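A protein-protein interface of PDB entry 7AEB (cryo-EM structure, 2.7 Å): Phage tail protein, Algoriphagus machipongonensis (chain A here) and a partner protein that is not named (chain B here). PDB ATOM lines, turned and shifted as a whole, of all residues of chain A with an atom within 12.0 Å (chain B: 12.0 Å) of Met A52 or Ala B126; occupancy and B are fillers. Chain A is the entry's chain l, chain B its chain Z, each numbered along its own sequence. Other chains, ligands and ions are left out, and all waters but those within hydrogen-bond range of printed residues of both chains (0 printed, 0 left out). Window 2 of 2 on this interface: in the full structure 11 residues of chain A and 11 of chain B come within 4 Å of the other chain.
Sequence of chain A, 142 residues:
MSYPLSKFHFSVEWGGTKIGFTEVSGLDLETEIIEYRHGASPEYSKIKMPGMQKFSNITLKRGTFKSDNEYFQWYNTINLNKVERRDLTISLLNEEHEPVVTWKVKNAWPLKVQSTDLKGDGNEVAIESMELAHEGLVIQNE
The backbone carbonyl oxygen of Glu B128 sits close to the side-chain sulfur of Met A52.
ND2 of Asn B125 sits close to OE1 of Glu B128, at 3.5 Å. The side-chain carboxylate (OE1) of Glu B128 is in salt-bridge range of the side-chain amino group (NZ) of Lys B130 (2.8 Å). The backbone carbonyl oxygen of Glu A32 sits at hydrogen-bond distance from the backbone NH of Gly A51, 2.8 Å away. N of Glu A32 sits at hydrogen-bond distance from O of Met A52 (3.0 Å). The backbone carbonyl oxygen of Met A49 lies within hydrogen-bond range of the backbone NH of Ile A34, at 2.9 Å.
Ile A34 touches Ser B129 (CD1 to OG, 3.4 Å). Met A49 touches Met B131 (CE to CE, 3.8 Å). CA of Gly A51 touches OG of Ser B129 (3.5 Å). Met A52 touches Ala B126 (CE to O, 3.6 Å). N of Met A52 touches OG of Ser B129, at 3.6 Å.
No residue of chain B comes within 4 Å of Glu A32. Of the printed residues of chain B, Ile A34 touches Ser B129 (3.4 Å). Of the printed residues of chain B, Met A49 touches Met B131 (3.8 Å). Of chain B, only Ser B129 (3.5 Å) comes within 4 Å of Gly A51. Met A52 touches just these residues of chain B: Ala B126 (3.6 Å), Glu B128 (3.6 Å) and Ser B129 (3.6 Å). No residue of chain B comes within 4 Å of Gln A53. No residue of chain B comes within 4 Å of Lys A54. Glu A135 touches none of the printed residues of chain B. Ala B126 touches just one residue of chain A: Met A52. No residue of chain A comes within 4 Å of Gln B127. Of the printed residues of chain A, Glu B128 touches Met A52. Printed residues of chain A within 4 Å of Ser B129: Ile A34, Gly A51 and Met A52. Printed residues of chain A within 4 Å of Met B131: Met A49 (3.8 Å). The nearest residue of chain A that does not touch Ala B126 is Gln A53 (9.1 Å). The nearest printed residue of chain B that does not touch Ile A34 is Met B131 (4.3 Å).
Printed residues of chain A that touch a printed residue of chain B: Ile A34, Met A49, Gly A51 and Met A52. Among the printed residues, 6 pairs touch across the chains. Among the printed residues, no Asp or Glu carboxylate lies within 4 Å of a Lys or Arg side-chain nitrogen of the other chain.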
ATOM      1  N   ASP A  28      -7.456  -0.710   3.550  1.00  0.00           N
ATOM      2  CA  ASP A  28      -8.660  -1.498   3.870  1.00  0.00           C
ATOM      3  C   ASP A  28     -10.003  -0.839   3.512  1.00  0.00           C
ATOM      4  O   ASP A  28     -10.108   0.385   3.445  1.00  0.00           O
ATOM      5  CB  ASP A  28      -8.695  -1.786   5.364  1.00  0.00           C
ATOM      6  CG  ASP A  28      -7.578  -2.660   5.861  1.00  0.00           C
ATOM      7  OD1 ASP A  28      -7.298  -3.657   5.253  1.00  0.00           O
ATOM      8  OD2 ASP A  28      -6.997  -2.315   6.869  1.00  0.00           O
ATOM      9  N   LEU A  29     -11.036  -1.675   3.333  1.00  0.00           N
ATOM     10  CA  LEU A  29     -12.432  -1.269   3.082  1.00  0.00           C
ATOM     11  C   LEU A  29     -13.358  -2.007   4.064  1.00  0.00           C
ATOM     12  O   LEU A  29     -13.209  -3.216   4.226  1.00  0.00           O
ATOM     13  CB  LEU A  29     -12.828  -1.669   1.650  1.00  0.00           C
ATOM     14  CG  LEU A  29     -11.996  -1.062   0.481  1.00  0.00           C
ATOM     15  CD1 LEU A  29     -12.354  -1.750  -0.805  1.00  0.00           C
ATOM     16  CD2 LEU A  29     -12.280   0.385   0.343  1.00  0.00           C
ATOM     17  N   GLU A  30     -14.338  -1.329   4.685  1.00  0.00           N
ATOM     18  CA  GLU A  30     -15.232  -2.025   5.633  1.00  0.00           C
ATOM     19  C   GLU A  30     -16.700  -1.549   5.634  1.00  0.00           C
ATOM     20  O   GLU A  30     -16.985  -0.357   5.545  1.00  0.00           O
ATOM     21  CB  GLU A  30     -14.641  -1.893   7.033  1.00  0.00           C
ATOM     22  CG  GLU A  30     -15.370  -2.625   8.124  1.00  0.00           C
ATOM     23  CD  GLU A  30     -14.680  -2.489   9.440  1.00  0.00           C
ATOM     24  OE1 GLU A  30     -13.597  -1.975   9.465  1.00  0.00           O
ATOM     25  OE2 GLU A  30     -15.251  -2.848  10.434  1.00  0.00           O
ATOM     26  N   THR A  31     -17.642  -2.498   5.745  1.00  0.00           N
ATOM     27  CA  THR A  31     -19.087  -2.194   5.789  1.00  0.00           C
ATOM     28  C   THR A  31     -19.769  -2.776   7.039  1.00  0.00           C
ATOM     29  O   THR A  31     -19.506  -3.920   7.413  1.00  0.00           O
ATOM     30  CB  THR A  31     -19.803  -2.732   4.520  1.00  0.00           C
ATOM     31  OG1 THR A  31     -19.218  -2.150   3.364  1.00  0.00           O
ATOM     32  CG2 THR A  31     -21.282  -2.354   4.524  1.00  0.00           C
ATOM     33  N   GLU A  32     -20.656  -1.992   7.658  1.00  0.00           N
ATOM     34  CA  GLU A  32     -21.448  -2.404   8.825  1.00  0.00           C
ATOM     35  C   GLU A  32     -22.625  -3.318   8.483  1.00  0.00           C
ATOM     36  O   GLU A  32     -23.108  -3.331   7.350  1.00  0.00           O
ATOM     37  CB  GLU A  32     -22.006  -1.180   9.537  1.00  0.00           C
ATOM     38  CG  GLU A  32     -20.985  -0.314  10.176  1.00  0.00           C
ATOM     39  CD  GLU A  32     -20.382  -0.982  11.346  1.00  0.00           C
ATOM     40  OE1 GLU A  32     -21.103  -1.608  12.073  1.00  0.00           O
ATOM     41  OE2 GLU A  32     -19.194  -0.890  11.526  1.00  0.00           O
ATOM     42  N   ILE A  33     -23.090  -4.078   9.469  1.00  0.00           N
ATOM     43  CA  ILE A  33     -24.200  -4.999   9.245  1.00  0.00           C
ATOM     44  C   ILE A  33     -25.431  -4.733  10.109  1.00  0.00           C
ATOM     45  O   ILE A  33     -25.334  -4.574  11.327  1.00  0.00           O
ATOM     46  CB  ILE A  33     -23.759  -6.462   9.450  1.00  0.00           C
ATOM     47  CG1 ILE A  33     -22.564  -6.789   8.553  1.00  0.00           C
ATOM     48  CG2 ILE A  33     -24.915  -7.411   9.169  1.00  0.00           C
ATOM     49  CD1 ILE A  33     -22.063  -8.210   8.695  1.00  0.00           C
ATOM     50  N   ILE A  34     -26.590  -4.690   9.459  1.00  0.00           N
ATOM     51  CA  ILE A  34     -27.866  -4.487  10.123  1.00  0.00           C
ATOM     52  C   ILE A  34     -28.605  -5.828  10.223  1.00  0.00           C
ATOM     53  O   ILE A  34     -28.797  -6.516   9.220  1.00  0.00           O
ATOM     54  CB  ILE A  34     -28.704  -3.455   9.356  1.00  0.00           C
ATOM     55  CG1 ILE A  34     -27.935  -2.121   9.316  1.00  0.00           C
ATOM     56  CG2 ILE A  34     -30.072  -3.299  10.029  1.00  0.00           C
ATOM     57  CD1 ILE A  34     -28.484  -1.112   8.366  1.00  0.00           C
ATOM     58  N   GLU A  35     -28.974  -6.226  11.444  1.00  0.00           N
ATOM     59  CA  GLU A  35     -29.626  -7.524  11.682  1.00  0.00           C
ATOM     60  C   GLU A  35     -31.120  -7.410  12.032  1.00  0.00           C
ATOM     61  O   GLU A  35     -31.528  -6.461  12.700  1.00  0.00           O
ATOM     62  CB  GLU A  35     -28.907  -8.253  12.812  1.00  0.00           C
ATOM     63  CG  GLU A  35     -27.456  -8.574  12.540  1.00  0.00           C
ATOM     64  CD  GLU A  35     -26.808  -9.331  13.657  1.00  0.00           C
ATOM     65  OE1 GLU A  35     -27.434  -9.469  14.678  1.00  0.00           O
ATOM     66  OE2 GLU A  35     -25.692  -9.777  13.501  1.00  0.00           O
ATOM     67  N   LYS A  48     -29.449 -10.725   7.586  1.00  0.00           N
ATOM     68  CA  LYS A  48     -28.485  -9.624   7.538  1.00  0.00           C
ATOM     69  C   LYS A  48     -28.475  -8.790   6.254  1.00  0.00           C
ATOM     70  O   LYS A  48     -28.574  -9.335   5.157  1.00  0.00           O
ATOM     71  CB  LYS A  48     -27.120 -10.263   7.718  1.00  0.00           C
ATOM     72  CG  LYS A  48     -27.000 -10.992   9.022  1.00  0.00           C
ATOM     73  CD  LYS A  48     -25.685 -11.658   9.211  1.00  0.00           C
ATOM     74  CE  LYS A  48     -25.681 -12.419  10.521  1.00  0.00           C
ATOM     75  NZ  LYS A  48     -24.407 -13.123  10.753  1.00  0.00           N
ATOM     76  N   MET A  49     -28.258  -7.476   6.397  1.00  0.00           N
ATOM     77  CA  MET A  49     -28.091  -6.601   5.230  1.00  0.00           C
ATOM     78  C   MET A  49     -27.022  -5.509   5.476  1.00  0.00           C
ATOM     79  O   MET A  49     -26.801  -5.126   6.621  1.00  0.00           O
ATOM     80  CB  MET A  49     -29.420  -5.948   4.851  1.00  0.00           C
ATOM     81  CG  MET A  49     -29.979  -5.004   5.867  1.00  0.00           C
ATOM     82  SD  MET A  49     -31.560  -4.330   5.367  1.00  0.00           S
ATOM     83  CE  MET A  49     -31.838  -3.152   6.663  1.00  0.00           C
ATOM     84  N   PRO A  50     -26.351  -4.976   4.436  1.00  0.00           N
ATOM     85  CA  PRO A  50     -25.389  -3.879   4.502  1.00  0.00           C
ATOM     86  C   PRO A  50     -25.888  -2.555   5.081  1.00  0.00           C
ATOM     87  O   PRO A  50     -26.966  -2.079   4.732  1.00  0.00           O
ATOM     88  CB  PRO A  50     -25.061  -3.657   3.026  1.00  0.00           C
ATOM     89  CG  PRO A  50     -25.328  -4.951   2.364  1.00  0.00           C
ATOM     90  CD  PRO A  50     -26.508  -5.524   3.073  1.00  0.00           C
ATOM     91  N   GLY A  51     -25.029  -1.959   5.892  1.00  0.00           N
ATOM     92  CA  GLY A  51     -25.136  -0.667   6.555  1.00  0.00           C
ATOM     93  C   GLY A  51     -24.201   0.372   5.924  1.00  0.00           C
ATOM     94  O   GLY A  51     -23.922   0.345   4.725  1.00  0.00           O
ATOM     95  N   MET A  52     -23.773   1.333   6.745  1.00  0.00           N
ATOM     96  CA  MET A  52     -22.873   2.419   6.354  1.00  0.00           C
ATOM     97  C   MET A  52     -21.425   1.934   6.201  1.00  0.00           C
ATOM     98  O   MET A  52     -21.052   0.887   6.741  1.00  0.00           O
ATOM     99  CB  MET A  52     -22.966   3.560   7.347  1.00  0.00           C
ATOM    100  CG  MET A  52     -24.321   4.258   7.329  1.00  0.00           C
ATOM    101  SD  MET A  52     -24.475   5.609   8.500  1.00  0.00           S
ATOM    102  CE  MET A  52     -23.479   6.881   7.735  1.00  0.00           C
ATOM    103  N   GLN A  53     -20.613   2.684   5.446  1.00  0.00           N
ATOM    104  CA  GLN A  53     -19.219   2.299   5.188  1.00  0.00           C
ATOM    105  C   GLN A  53     -18.143   3.112   5.921  1.00  0.00           C
ATOM    106  O   GLN A  53     -18.344   4.278   6.260  1.00  0.00           O
ATOM    107  CB  GLN A  53     -18.975   2.371   3.692  1.00  0.00           C
ATOM    108  CG  GLN A  53     -19.861   1.429   2.911  1.00  0.00           C
ATOM    109  CD  GLN A  53     -19.619   1.480   1.439  1.00  0.00           C
ATOM    110  OE1 GLN A  53     -18.981   2.409   0.942  1.00  0.00           O
ATOM    111  NE2 GLN A  53     -20.129   0.494   0.722  1.00  0.00           N
ATOM    112  N   LYS A  54     -16.989   2.464   6.130  1.00  0.00           N
ATOM    113  CA  LYS A  54     -15.783   3.009   6.763  1.00  0.00           C
ATOM    114  C   LYS A  54     -14.495   2.809   5.969  1.00  0.00           C
ATOM    115  O   LYS A  54     -14.366   1.889   5.153  1.00  0.00           O
ATOM    116  CB  LYS A  54     -15.551   2.355   8.109  1.00  0.00           C
ATOM    117  CG  LYS A  54     -16.572   2.632   9.151  1.00  0.00           C
ATOM    118  CD  LYS A  54     -16.314   1.789  10.391  1.00  0.00           C
ATOM    119  CE  LYS A  54     -16.830   0.362  10.187  1.00  0.00           C
ATOM    120  NZ  LYS A  54     -16.743  -0.477  11.422  1.00  0.00           N
ATOM    121  N   PHE A  55     -13.510   3.656   6.275  1.00  0.00           N
ATOM    122  CA  PHE A  55     -12.162   3.518   5.734  1.00  0.00           C
ATOM    123  C   PHE A  55     -11.133   3.594   6.856  1.00  0.00           C
ATOM    124  O   PHE A  55     -11.348   4.294   7.843  1.00  0.00           O
ATOM    125  CB  PHE A  55     -11.873   4.612   4.722  1.00  0.00           C
ATOM    126  CG  PHE A  55     -12.783   4.588   3.568  1.00  0.00           C
ATOM    127  CD1 PHE A  55     -13.865   5.434   3.521  1.00  0.00           C
ATOM    128  CD2 PHE A  55     -12.601   3.688   2.549  1.00  0.00           C
ATOM    129  CE1 PHE A  55     -14.739   5.385   2.486  1.00  0.00           C
ATOM    130  CE2 PHE A  55     -13.480   3.640   1.511  1.00  0.00           C
ATOM    131  CZ  PHE A  55     -14.550   4.483   1.479  1.00  0.00           C
ATOM    132  N   SER A  56     -10.010   2.899   6.700  1.00  0.00           N
ATOM    133  CA  SER A  56      -8.903   2.960   7.667  1.00  0.00           C
ATOM    134  C   SER A  56      -7.905   4.063   7.332  1.00  0.00           C
ATOM    135  O   SER A  56      -7.793   4.477   6.175  1.00  0.00           O
ATOM    136  CB  SER A  56      -8.157   1.639   7.722  1.00  0.00           C
ATOM    137  OG  SER A  56      -8.965   0.607   8.209  1.00  0.00           O
ATOM    138  N   GLU A 135     -10.896  10.206   2.431  1.00  0.00           N
ATOM    139  CA  GLU A 135     -12.326  10.024   2.189  1.00  0.00           C
ATOM    140  C   GLU A 135     -12.717   8.966   1.151  1.00  0.00           C
ATOM    141  O   GLU A 135     -13.817   9.034   0.599  1.00  0.00           O
ATOM    142  CB  GLU A 135     -12.958  11.370   1.815  1.00  0.00           C
ATOM    143  CG  GLU A 135     -12.918  12.411   2.940  1.00  0.00           C
ATOM    144  CD  GLU A 135     -13.570  13.725   2.590  1.00  0.00           C
ATOM    145  OE1 GLU A 135     -13.927  13.907   1.458  1.00  0.00           O
ATOM    146  OE2 GLU A 135     -13.699  14.548   3.459  1.00  0.00           O
ATOM    147  N   GLU B 122     -39.816   6.194  14.326  1.00  0.00           N
ATOM    148  CA  GLU B 122     -38.655   6.718  15.037  1.00  0.00           C
ATOM    149  C   GLU B 122     -37.799   7.658  14.181  1.00  0.00           C
ATOM    150  O   GLU B 122     -37.765   7.561  12.953  1.00  0.00           O
ATOM    151  CB  GLU B 122     -37.794   5.567  15.559  1.00  0.00           C
ATOM    152  CG  GLU B 122     -38.496   4.756  16.626  1.00  0.00           C
ATOM    153  CD  GLU B 122     -37.622   3.737  17.282  1.00  0.00           C
ATOM    154  OE1 GLU B 122     -36.491   3.552  16.839  1.00  0.00           O
ATOM    155  OE2 GLU B 122     -38.105   3.047  18.187  1.00  0.00           O
ATOM    156  N   ASP B 123     -37.076   8.550  14.870  1.00  0.00           N
ATOM    157  CA  ASP B 123     -36.247   9.610  14.288  1.00  0.00           C
ATOM    158  C   ASP B 123     -35.197   9.115  13.300  1.00  0.00           C
ATOM    159  O   ASP B 123     -34.569   8.072  13.481  1.00  0.00           O
ATOM    160  CB  ASP B 123     -35.466  10.347  15.369  1.00  0.00           C
ATOM    161  CG  ASP B 123     -36.307  11.199  16.271  1.00  0.00           C
ATOM    162  OD1 ASP B 123     -37.492  11.395  16.031  1.00  0.00           O
ATOM    163  OD2 ASP B 123     -35.751  11.689  17.254  1.00  0.00           O
ATOM    164  N   PHE B 124     -34.951   9.942  12.298  1.00  0.00           N
ATOM    165  CA  PHE B 124     -33.943   9.685  11.287  1.00  0.00           C
ATOM    166  C   PHE B 124     -32.624  10.288  11.745  1.00  0.00           C
ATOM    167  O   PHE B 124     -32.610  11.340  12.378  1.00  0.00           O
ATOM    168  CB  PHE B 124     -34.363  10.313   9.963  1.00  0.00           C
ATOM    169  CG  PHE B 124     -35.654   9.771   9.387  1.00  0.00           C
ATOM    170  CD1 PHE B 124     -36.328  10.511   8.447  1.00  0.00           C
ATOM    171  CD2 PHE B 124     -36.199   8.545   9.771  1.00  0.00           C
ATOM    172  CE1 PHE B 124     -37.508  10.061   7.900  1.00  0.00           C
ATOM    173  CE2 PHE B 124     -37.382   8.103   9.230  1.00  0.00           C
ATOM    174  CZ  PHE B 124     -38.032   8.860   8.291  1.00  0.00           C
ATOM    175  N   ASN B 125     -31.513   9.626  11.424  1.00  0.00           N
ATOM    176  CA  ASN B 125     -30.198  10.138  11.809  1.00  0.00           C
ATOM    177  C   ASN B 125     -29.186   9.795  10.727  1.00  0.00           C
ATOM    178  O   ASN B 125     -28.840   8.634  10.526  1.00  0.00           O
ATOM    179  CB  ASN B 125     -29.781   9.586  13.166  1.00  0.00           C
ATOM    180  CG  ASN B 125     -28.507  10.218  13.708  1.00  0.00           C
ATOM    181  OD1 ASN B 125     -27.593  10.640  12.991  1.00  0.00           O
ATOM    182  ND2 ASN B 125     -28.438  10.274  15.011  1.00  0.00           N
ATOM    183  N   ALA B 126     -28.672  10.840  10.083  1.00  0.00           N
ATOM    184  CA  ALA B 126     -27.736  10.721   8.973  1.00  0.00           C
ATOM    185  C   ALA B 126     -26.413  10.077   9.352  1.00  0.00           C
ATOM    186  O   ALA B 126     -25.676   9.631   8.469  1.00  0.00           O
ATOM    187  CB  ALA B 126     -27.449  12.098   8.410  1.00  0.00           C
ATOM    188  N   GLN B 127     -26.065  10.075  10.631  1.00  0.00           N
ATOM    189  CA  GLN B 127     -24.787   9.556  11.080  1.00  0.00           C
ATOM    190  C   GLN B 127     -24.878   8.190  11.756  1.00  0.00           C
ATOM    191  O   GLN B 127     -23.888   7.741  12.333  1.00  0.00           O
ATOM    192  CB  GLN B 127     -24.129  10.564  12.015  1.00  0.00           C
ATOM    193  CG  GLN B 127     -23.775  11.859  11.319  1.00  0.00           C
ATOM    194  CD  GLN B 127     -23.114  12.858  12.221  1.00  0.00           C
ATOM    195  OE1 GLN B 127     -22.299  12.503  13.069  1.00  0.00           O
ATOM    196  NE2 GLN B 127     -23.458  14.122  12.049  1.00  0.00           N
ATOM    197  N   GLU B 128     -26.020   7.504  11.689  1.00  0.00           N
ATOM    198  CA  GLU B 128     -26.128   6.212  12.347  1.00  0.00           C
ATOM    199  C   GLU B 128     -26.644   5.161  11.363  1.00  0.00           C
ATOM    200  O   GLU B 128     -27.457   5.455  10.489  1.00  0.00           O
ATOM    201  CB  GLU B 128     -27.095   6.300  13.513  1.00  0.00           C
ATOM    202  CG  GLU B 128     -26.586   7.081  14.702  1.00  0.00           C
ATOM    203  CD  GLU B 128     -27.576   7.073  15.833  1.00  0.00           C
ATOM    204  OE1 GLU B 128     -28.765   6.872  15.578  1.00  0.00           O
ATOM    205  OE2 GLU B 128     -27.165   7.201  16.991  1.00  0.00           O
ATOM    206  N   SER B 129     -26.189   3.936  11.515  1.00  0.00           N
ATOM    207  CA  SER B 129     -26.694   2.809  10.737  1.00  0.00           C
ATOM    208  C   SER B 129     -27.796   2.069  11.457  1.00  0.00           C
ATOM    209  O   SER B 129     -27.524   1.274  12.354  1.00  0.00           O
ATOM    210  CB  SER B 129     -25.562   1.861  10.407  1.00  0.00           C
ATOM    211  OG  SER B 129     -26.014   0.854   9.545  1.00  0.00           O
ATOM    212  N   LYS B 130     -29.047   2.331  11.068  1.00  0.00           N
ATOM    213  CA  LYS B 130     -30.212   1.791  11.755  1.00  0.00           C
ATOM    214  C   LYS B 130     -31.363   1.535  10.792  1.00  0.00           C
ATOM    215  O   LYS B 130     -31.461   2.147   9.732  1.00  0.00           O
ATOM    216  CB  LYS B 130     -30.680   2.755  12.841  1.00  0.00           C
ATOM    217  CG  LYS B 130     -29.795   2.824  14.053  1.00  0.00           C
ATOM    218  CD  LYS B 130     -30.346   3.736  15.096  1.00  0.00           C
ATOM    219  CE  LYS B 130     -29.371   3.881  16.253  1.00  0.00           C
ATOM    220  NZ  LYS B 130     -29.821   4.912  17.231  1.00  0.00           N
ATOM    221  N   MET B 131     -32.254   0.641  11.202  1.00  0.00           N
ATOM    222  CA  MET B 131     -33.473   0.342  10.468  1.00  0.00           C
ATOM    223  C   MET B 131     -34.577   1.302  10.880  1.00  0.00           C
ATOM    224  O   MET B 131     -34.669   1.676  12.045  1.00  0.00           O
ATOM    225  CB  MET B 131     -33.893  -1.096  10.760  1.00  0.00           C
ATOM    226  CG  MET B 131     -35.116  -1.567  10.026  1.00  0.00           C
ATOM    227  SD  MET B 131     -35.502  -3.269  10.371  1.00  0.00           S
ATOM    228  CE  MET B 131     -34.271  -4.130   9.407  1.00  0.00           C
ATOM    229  N   ALA B 132     -35.428   1.691   9.935  1.00  0.00           N
ATOM    230  CA  ALA B 132     -36.580   2.507  10.292  1.00  0.00           C
ATOM    231  C   ALA B 132     -37.635   1.644  10.971  1.00  0.00           C
ATOM    232  O   ALA B 132     -38.080   0.642  10.407  1.00  0.00           O
ATOM    233  CB  ALA B 132     -37.162   3.192   9.065  1.00  0.00           C
